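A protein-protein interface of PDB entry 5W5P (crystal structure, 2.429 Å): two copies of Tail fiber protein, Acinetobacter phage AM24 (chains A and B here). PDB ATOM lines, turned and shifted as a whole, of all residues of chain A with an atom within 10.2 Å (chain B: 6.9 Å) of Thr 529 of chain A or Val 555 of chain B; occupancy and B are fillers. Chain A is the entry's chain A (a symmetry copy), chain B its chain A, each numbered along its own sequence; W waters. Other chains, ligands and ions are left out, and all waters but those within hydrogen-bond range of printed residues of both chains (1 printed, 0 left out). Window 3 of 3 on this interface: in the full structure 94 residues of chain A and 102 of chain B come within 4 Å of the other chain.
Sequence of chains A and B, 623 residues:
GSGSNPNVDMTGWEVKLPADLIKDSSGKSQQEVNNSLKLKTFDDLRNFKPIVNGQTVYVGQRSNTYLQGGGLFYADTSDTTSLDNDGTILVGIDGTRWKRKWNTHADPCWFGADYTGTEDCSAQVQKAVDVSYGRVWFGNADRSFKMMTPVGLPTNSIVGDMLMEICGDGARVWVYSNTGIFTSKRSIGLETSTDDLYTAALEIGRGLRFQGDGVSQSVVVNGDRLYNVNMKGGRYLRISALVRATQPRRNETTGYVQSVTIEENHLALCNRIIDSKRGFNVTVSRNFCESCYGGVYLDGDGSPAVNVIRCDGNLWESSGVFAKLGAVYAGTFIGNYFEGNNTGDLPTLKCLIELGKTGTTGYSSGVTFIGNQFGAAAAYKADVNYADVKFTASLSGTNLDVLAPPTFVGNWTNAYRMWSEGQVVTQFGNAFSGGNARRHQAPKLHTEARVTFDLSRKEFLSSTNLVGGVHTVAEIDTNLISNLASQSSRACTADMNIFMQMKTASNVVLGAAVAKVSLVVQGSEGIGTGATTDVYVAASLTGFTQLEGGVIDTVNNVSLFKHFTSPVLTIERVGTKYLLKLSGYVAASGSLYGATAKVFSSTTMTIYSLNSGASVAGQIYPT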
ATOM      1  N   GLN A 487      22.381 -34.496  15.262  1.00  0.00           N
ATOM      2  CA  GLN A 487      20.964 -34.161  15.361  1.00  0.00           C
ATOM      3  C   GLN A 487      20.097 -35.212  14.681  1.00  0.00           C
ATOM      4  O   GLN A 487      19.034 -35.575  15.197  1.00  0.00           O
ATOM      5  CB  GLN A 487      20.702 -32.780  14.755  1.00  0.00           C
ATOM      6  CG  GLN A 487      21.055 -31.617  15.673  1.00  0.00           C
ATOM      7  CD  GLN A 487      20.862 -30.270  15.004  1.00  0.00           C
ATOM      8  OE1 GLN A 487      20.761 -30.181  13.779  1.00  0.00           O
ATOM      9  NE2 GLN A 487      20.825 -29.209  15.803  1.00  0.00           N
ATOM     10  N   SER A 524      15.843 -30.237  17.765  1.00  0.00           N
ATOM     11  CA  SER A 524      16.433 -29.426  16.708  1.00  0.00           C
ATOM     12  C   SER A 524      17.101 -30.323  15.670  1.00  0.00           C
ATOM     13  O   SER A 524      17.892 -31.208  16.014  1.00  0.00           O
ATOM     14  CB  SER A 524      17.448 -28.449  17.300  1.00  0.00           C
ATOM     15  OG  SER A 524      16.882 -27.716  18.374  1.00  0.00           O
ATOM     16  N   GLU A 525      16.783 -30.093  14.396  1.00  0.00           N
ATOM     17  CA  GLU A 525      17.326 -30.888  13.298  1.00  0.00           C
ATOM     18  C   GLU A 525      17.531 -29.981  12.095  1.00  0.00           C
ATOM     19  O   GLU A 525      16.579 -29.355  11.620  1.00  0.00           O
ATOM     20  CB  GLU A 525      16.395 -32.048  12.944  1.00  0.00           C
ATOM     21  CG  GLU A 525      16.975 -33.038  11.953  1.00  0.00           C
ATOM     22  CD  GLU A 525      16.429 -34.441  12.147  1.00  0.00           C
ATOM     23  OE1 GLU A 525      15.540 -34.616  13.007  1.00  0.00           O
ATOM     24  OE2 GLU A 525      16.891 -35.367  11.444  1.00  0.00           O
ATOM     25  N   GLY A 526      18.768 -29.918  11.603  1.00  0.00           N
ATOM     26  CA  GLY A 526      19.107 -29.032  10.508  1.00  0.00           C
ATOM     27  C   GLY A 526      19.361 -27.599  10.911  1.00  0.00           C
ATOM     28  O   GLY A 526      19.344 -26.709  10.052  1.00  0.00           O
ATOM     29  N   ILE A 527      19.606 -27.345  12.195  1.00  0.00           N
ATOM     30  CA  ILE A 527      19.681 -25.999  12.744  1.00  0.00           C
ATOM     31  C   ILE A 527      21.073 -25.776  13.315  1.00  0.00           C
ATOM     32  O   ILE A 527      21.541 -26.562  14.147  1.00  0.00           O
ATOM     33  CB  ILE A 527      18.608 -25.774  13.825  1.00  0.00           C
ATOM     34  CG1 ILE A 527      17.212 -25.839  13.205  1.00  0.00           C
ATOM     35  CG2 ILE A 527      18.824 -24.444  14.528  1.00  0.00           C
ATOM     36  CD1 ILE A 527      16.104 -25.793  14.224  1.00  0.00           C
ATOM     37  N   GLY A 528      21.726 -24.705  12.876  1.00  0.00           N
ATOM     38  CA  GLY A 528      23.018 -24.332  13.414  1.00  0.00           C
ATOM     39  C   GLY A 528      22.897 -23.398  14.599  1.00  0.00           C
ATOM     40  O   GLY A 528      22.876 -23.841  15.751  1.00  0.00           O
ATOM     41  N   THR A 529      22.802 -22.099  14.331  1.00  0.00           N
ATOM     42  CA  THR A 529      22.685 -21.120  15.404  1.00  0.00           C
ATOM     43  C   THR A 529      21.351 -21.283  16.125  1.00  0.00           C
ATOM     44  O   THR A 529      20.292 -21.315  15.492  1.00  0.00           O
ATOM     45  CB  THR A 529      22.816 -19.705  14.845  1.00  0.00           C
ATOM     46  OG1 THR A 529      24.093 -19.564  14.211  1.00  0.00           O
ATOM     47  CG2 THR A 529      22.703 -18.682  15.962  1.00  0.00           C
ATOM     48  N   GLY A 530      21.410 -21.404  17.451  1.00  0.00           N
ATOM     49  CA  GLY A 530      20.222 -21.493  18.277  1.00  0.00           C
ATOM     50  C   GLY A 530      19.733 -22.893  18.574  1.00  0.00           C
ATOM     51  O   GLY A 530      18.750 -23.044  19.314  1.00  0.00           O
ATOM     52  N   ALA A 531      20.379 -23.921  18.029  1.00  0.00           N
ATOM     53  CA  ALA A 531      19.927 -25.287  18.247  1.00  0.00           C
ATOM     54  C   ALA A 531      20.114 -25.695  19.704  1.00  0.00           C
ATOM     55  O   ALA A 531      21.014 -25.218  20.399  1.00  0.00           O
ATOM     56  CB  ALA A 531      20.678 -26.253  17.330  1.00  0.00           C
ATOM     57  N   THR A 532      19.246 -26.587  20.164  1.00  0.00           N
ATOM     58  CA  THR A 532      19.308 -27.105  21.520  1.00  0.00           C
ATOM     59  C   THR A 532      19.403 -28.622  21.481  1.00  0.00           C
ATOM     60  O   THR A 532      19.008 -29.266  20.504  1.00  0.00           O
ATOM     61  CB  THR A 532      18.082 -26.692  22.344  1.00  0.00           C
ATOM     62  OG1 THR A 532      18.141 -27.317  23.632  1.00  0.00           O
ATOM     63  CG2 THR A 532      16.813 -27.129  21.640  1.00  0.00           C
ATOM     64  N   VAL B 551      10.955 -25.613  21.772  1.00  0.00           N
ATOM     65  CA  VAL B 551      11.921 -24.681  21.199  1.00  0.00           C
ATOM     66  C   VAL B 551      12.980 -25.457  20.425  1.00  0.00           C
ATOM     67  O   VAL B 551      13.632 -26.356  20.967  1.00  0.00           O
ATOM     68  CB  VAL B 551      12.567 -23.820  22.293  1.00  0.00           C
ATOM     69  CG1 VAL B 551      13.457 -22.755  21.671  1.00  0.00           C
ATOM     70  CG2 VAL B 551      11.504 -23.194  23.173  1.00  0.00           C
ATOM     71  N   ILE B 552      13.161 -25.103  19.154  1.00  0.00           N
ATOM     72  CA  ILE B 552      14.221 -25.676  18.331  1.00  0.00           C
ATOM     73  C   ILE B 552      15.281 -24.658  17.947  1.00  0.00           C
ATOM     74  O   ILE B 552      16.337 -25.055  17.428  1.00  0.00           O
ATOM     75  CB  ILE B 552      13.651 -26.344  17.061  1.00  0.00           C
ATOM     76  CG1 ILE B 552      12.858 -25.329  16.235  1.00  0.00           C
ATOM     77  CG2 ILE B 552      12.780 -27.537  17.433  1.00  0.00           C
ATOM     78  CD1 ILE B 552      12.208 -25.922  15.005  1.00  0.00           C
ATOM     79  N   ASP B 553      15.041 -23.365  18.182  1.00  0.00           N
ATOM     80  CA  ASP B 553      15.988 -22.299  17.843  1.00  0.00           C
ATOM     81  C   ASP B 553      15.846 -21.217  18.917  1.00  0.00           C
ATOM     82  O   ASP B 553      15.017 -20.312  18.798  1.00  0.00           O
ATOM     83  CB  ASP B 553      15.731 -21.747  16.448  1.00  0.00           C
ATOM     84  CG  ASP B 553      16.699 -20.635  16.060  1.00  0.00           C
ATOM     85  OD1 ASP B 553      17.637 -20.337  16.825  1.00  0.00           O
ATOM     86  OD2 ASP B 553      16.520 -20.053  14.973  1.00  0.00           O
ATOM     87  N   THR B 554      16.677 -21.318  19.956  1.00  0.00           N
ATOM     88  CA  THR B 554      16.607 -20.401  21.087  1.00  0.00           C
ATOM     89  C   THR B 554      17.071 -18.991  20.746  1.00  0.00           C
ATOM     90  O   THR B 554      16.846 -18.075  21.547  1.00  0.00           O
ATOM     91  CB  THR B 554      17.443 -20.941  22.243  1.00  0.00           C
ATOM     92  OG1 THR B 554      18.829 -20.899  21.882  1.00  0.00           O
ATOM     93  CG2 THR B 554      17.053 -22.378  22.546  1.00  0.00           C
ATOM     94  N   VAL B 555      17.713 -18.791  19.596  1.00  0.00           N
ATOM     95  CA  VAL B 555      18.160 -17.456  19.214  1.00  0.00           C
ATOM     96  C   VAL B 555      17.034 -16.692  18.529  1.00  0.00           C
ATOM     97  O   VAL B 555      16.753 -15.534  18.862  1.00  0.00           O
ATOM     98  CB  VAL B 555      19.411 -17.549  18.320  1.00  0.00           C
ATOM     99  CG1 VAL B 555      19.630 -16.246  17.563  1.00  0.00           C
ATOM    100  CG2 VAL B 555      20.635 -17.907  19.156  1.00  0.00           C
ATOM    101  N   ASN B 556      16.365 -17.328  17.570  1.00  0.00           N
ATOM    102  CA  ASN B 556      15.284 -16.704  16.822  1.00  0.00           C
ATOM    103  C   ASN B 556      13.906 -17.055  17.368  1.00  0.00           C
ATOM    104  O   ASN B 556      12.904 -16.566  16.835  1.00  0.00           O
ATOM    105  CB  ASN B 556      15.377 -17.095  15.343  1.00  0.00           C
ATOM    106  CG  ASN B 556      16.700 -16.688  14.715  1.00  0.00           C
ATOM    107  OD1 ASN B 556      17.437 -17.525  14.192  1.00  0.00           O
ATOM    108  ND2 ASN B 556      17.006 -15.397  14.765  1.00  0.00           N
ATOM    109  N   ASN B 557      13.836 -17.887  18.412  1.00  0.00           N
ATOM    110  CA  ASN B 557      12.589 -18.262  19.082  1.00  0.00           C
ATOM    111  C   ASN B 557      11.624 -18.945  18.106  1.00  0.00           C
ATOM    112  O   ASN B 557      10.537 -18.452  17.801  1.00  0.00           O
ATOM    113  CB  ASN B 557      11.933 -17.043  19.749  1.00  0.00           C
ATOM    114  CG  ASN B 557      12.818 -16.413  20.806  1.00  0.00           C
ATOM    115  OD1 ASN B 557      13.122 -17.033  21.827  1.00  0.00           O
ATOM    116  ND2 ASN B 557      13.240 -15.174  20.569  1.00  0.00           N
ATOM    117  N   VAL B 558      12.054 -20.112  17.634  1.00  0.00           N
ATOM    118  CA  VAL B 558      11.275 -20.931  16.713  1.00  0.00           C
ATOM    119  C   VAL B 558      10.949 -22.244  17.411  1.00  0.00           C
ATOM    120  O   VAL B 558      11.827 -22.863  18.022  1.00  0.00           O
ATOM    121  CB  VAL B 558      12.032 -21.173  15.393  1.00  0.00           C
ATOM    122  CG1 VAL B 558      11.220 -22.044  14.455  1.00  0.00           C
ATOM    123  CG2 VAL B 558      12.369 -19.846  14.727  1.00  0.00           C
ATOM    124  N   TYR B 593      13.407 -19.795   8.772  1.00  0.00           N
ATOM    125  CA  TYR B 593      13.680 -20.927   7.897  1.00  0.00           C
ATOM    126  C   TYR B 593      12.695 -21.059   6.744  1.00  0.00           C
ATOM    127  O   TYR B 593      12.903 -21.902   5.865  1.00  0.00           O
ATOM    128  CB  TYR B 593      13.692 -22.221   8.715  1.00  0.00           C
ATOM    129  CG  TYR B 593      14.612 -22.151   9.909  1.00  0.00           C
ATOM    130  CD1 TYR B 593      15.988 -22.249   9.753  1.00  0.00           C
ATOM    131  CD2 TYR B 593      14.108 -21.969  11.189  1.00  0.00           C
ATOM    132  CE1 TYR B 593      16.838 -22.177  10.839  1.00  0.00           C
ATOM    133  CE2 TYR B 593      14.952 -21.895  12.283  1.00  0.00           C
ATOM    134  CZ  TYR B 593      16.316 -22.003  12.100  1.00  0.00           C
ATOM    135  OH  TYR B 593      17.161 -21.936  13.182  1.00  0.00           O
HETATM  136  O   HOH W   1      20.992 -22.577  21.942  1.00  0.00           O
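The backbone carbonyl oxygen (O) of Ile 552 of chain B sits at hydrogen-bond distance from the side-chain hydroxyl (OG) of Ser 524 of chain A, 2.9 Å away. The backbone NH of Thr 554 of chain B sits at hydrogen-bond distance from the backbone carbonyl oxygen of Gly 530 of chain A (2.8 Å). The backbone carbonyl oxygen (O) of Thr 529 of chain A sits close to the side-chain carboxylate (OD1) of Asp 553 of chain B (3.1 Å).
N of Ile 552 of chain B is in hydrogen-bond range of O of Val 558 of chain B, at 2.8 Å. The side-chain carboxylate (OD1) of Asp 553 of chain B sits close to the backbone NH (N) of Val 555 of chain B (3.2 Å). N of Val 558 of chain B sits at hydrogen-bond distance from O of Asp 553 of chain B (3.2 Å). OD2 of Asp 553 of chain B is in hydrogen-bond range of OH of Tyr 593 of chain B (2.7 Å). The backbone carbonyl oxygen of Ile 527 of chain A sits at hydrogen-bond distance from the side-chain amide nitrogen of Gln 487 of chain A (3.2 Å). The side-chain hydroxyl (OG) of Ser 524 of chain A is in hydrogen-bond range of the backbone NH (N) of Thr 532 of chain A.
Among the printed residues, merely in contact across the chains: Gly 530 of chain A with Asp 553 of chain B, Ile 527 of chain A with Ile 552 of chain B, Ile 527 of chain A with Tyr 593 of chain B, Thr 532 of chain A with Val 551 of chain B, Gly 530 of chain A with Ile 552 of chain B, Ala 531 of chain A with Ile 552 of chain B, Gly 530 of chain A with Val 555 of chain B, Thr 529 of chain A with Val 555 of chain B and Thr 529 of chain A with Tyr 593 of chain B.
Printed residues of chain B within 4 Å of Ile 527 of chain A: Ile 552 (3.3 Å) and Tyr 593 (3.3 Å). Thr 529 of chain A touches three residues of chain B. Of the printed residues of chain B, Gly 530 of chain A touches Ile 552, Asp 553, Thr 554 and Val 555. Printed residues of chain B within 4 Å of Ala 531 of chain A: Ile 552. Printed residues of chain A within 4 Å of Val 551 of chain B: Thr 532 (3.3 Å). Of chain A, only Thr 529 (3.1 Å) and Gly 530 (3.2 Å) come within 4 Å of Asp 553 of chain B. Of the printed residues of chain A, Val 555 of chain B touches Thr 529 and Gly 530. No residue of chain A comes within 4 Å of Asn 556 of chain B. Val 558 of chain B touches none of the printed residues of chain A. The nearest residue of chain A that does not touch Val 555 of chain B is Ala 531 of chain A (6.0 Å). The nearest printed residue of chain A that does not touch Tyr 593 of chain B is Gly 526 of chain A (5.2 Å).
Printed residues of chain A that touch a printed residue of chain B: Ser 524, Ile 527, Thr 529, Gly 530, Ala 531 and Thr 532. Hydrophobic or aromatic side chains of chain A within 4 Å of the printed part of chain B: Ile 527. Of the 9 printed residues of chain B, 6 touch a printed residue of chain A. Hydrophobic or aromatic side chains of chain B within 4 Å of the printed part of chain A: Ile 552, Val 555 and Tyr 593. Along chain B the printed residues that touch a printed residue of chain A span positions 551 to 593. Among the printed residues, 12 pairs touch across the chains. Among the printed residues, no Asp or Glu carboxylate lies within 4 Å of a Lys or Arg side-chain nitrogen of the other chain.
No position is printed for both chains.
Water W1 lies within hydrogen-bond range of OG1 of Thr 554 of chain B (2.7 Å), O of Ala 531 of chain A (3.1 Å) and O of Gly 530 of chain A (3.5 Å).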
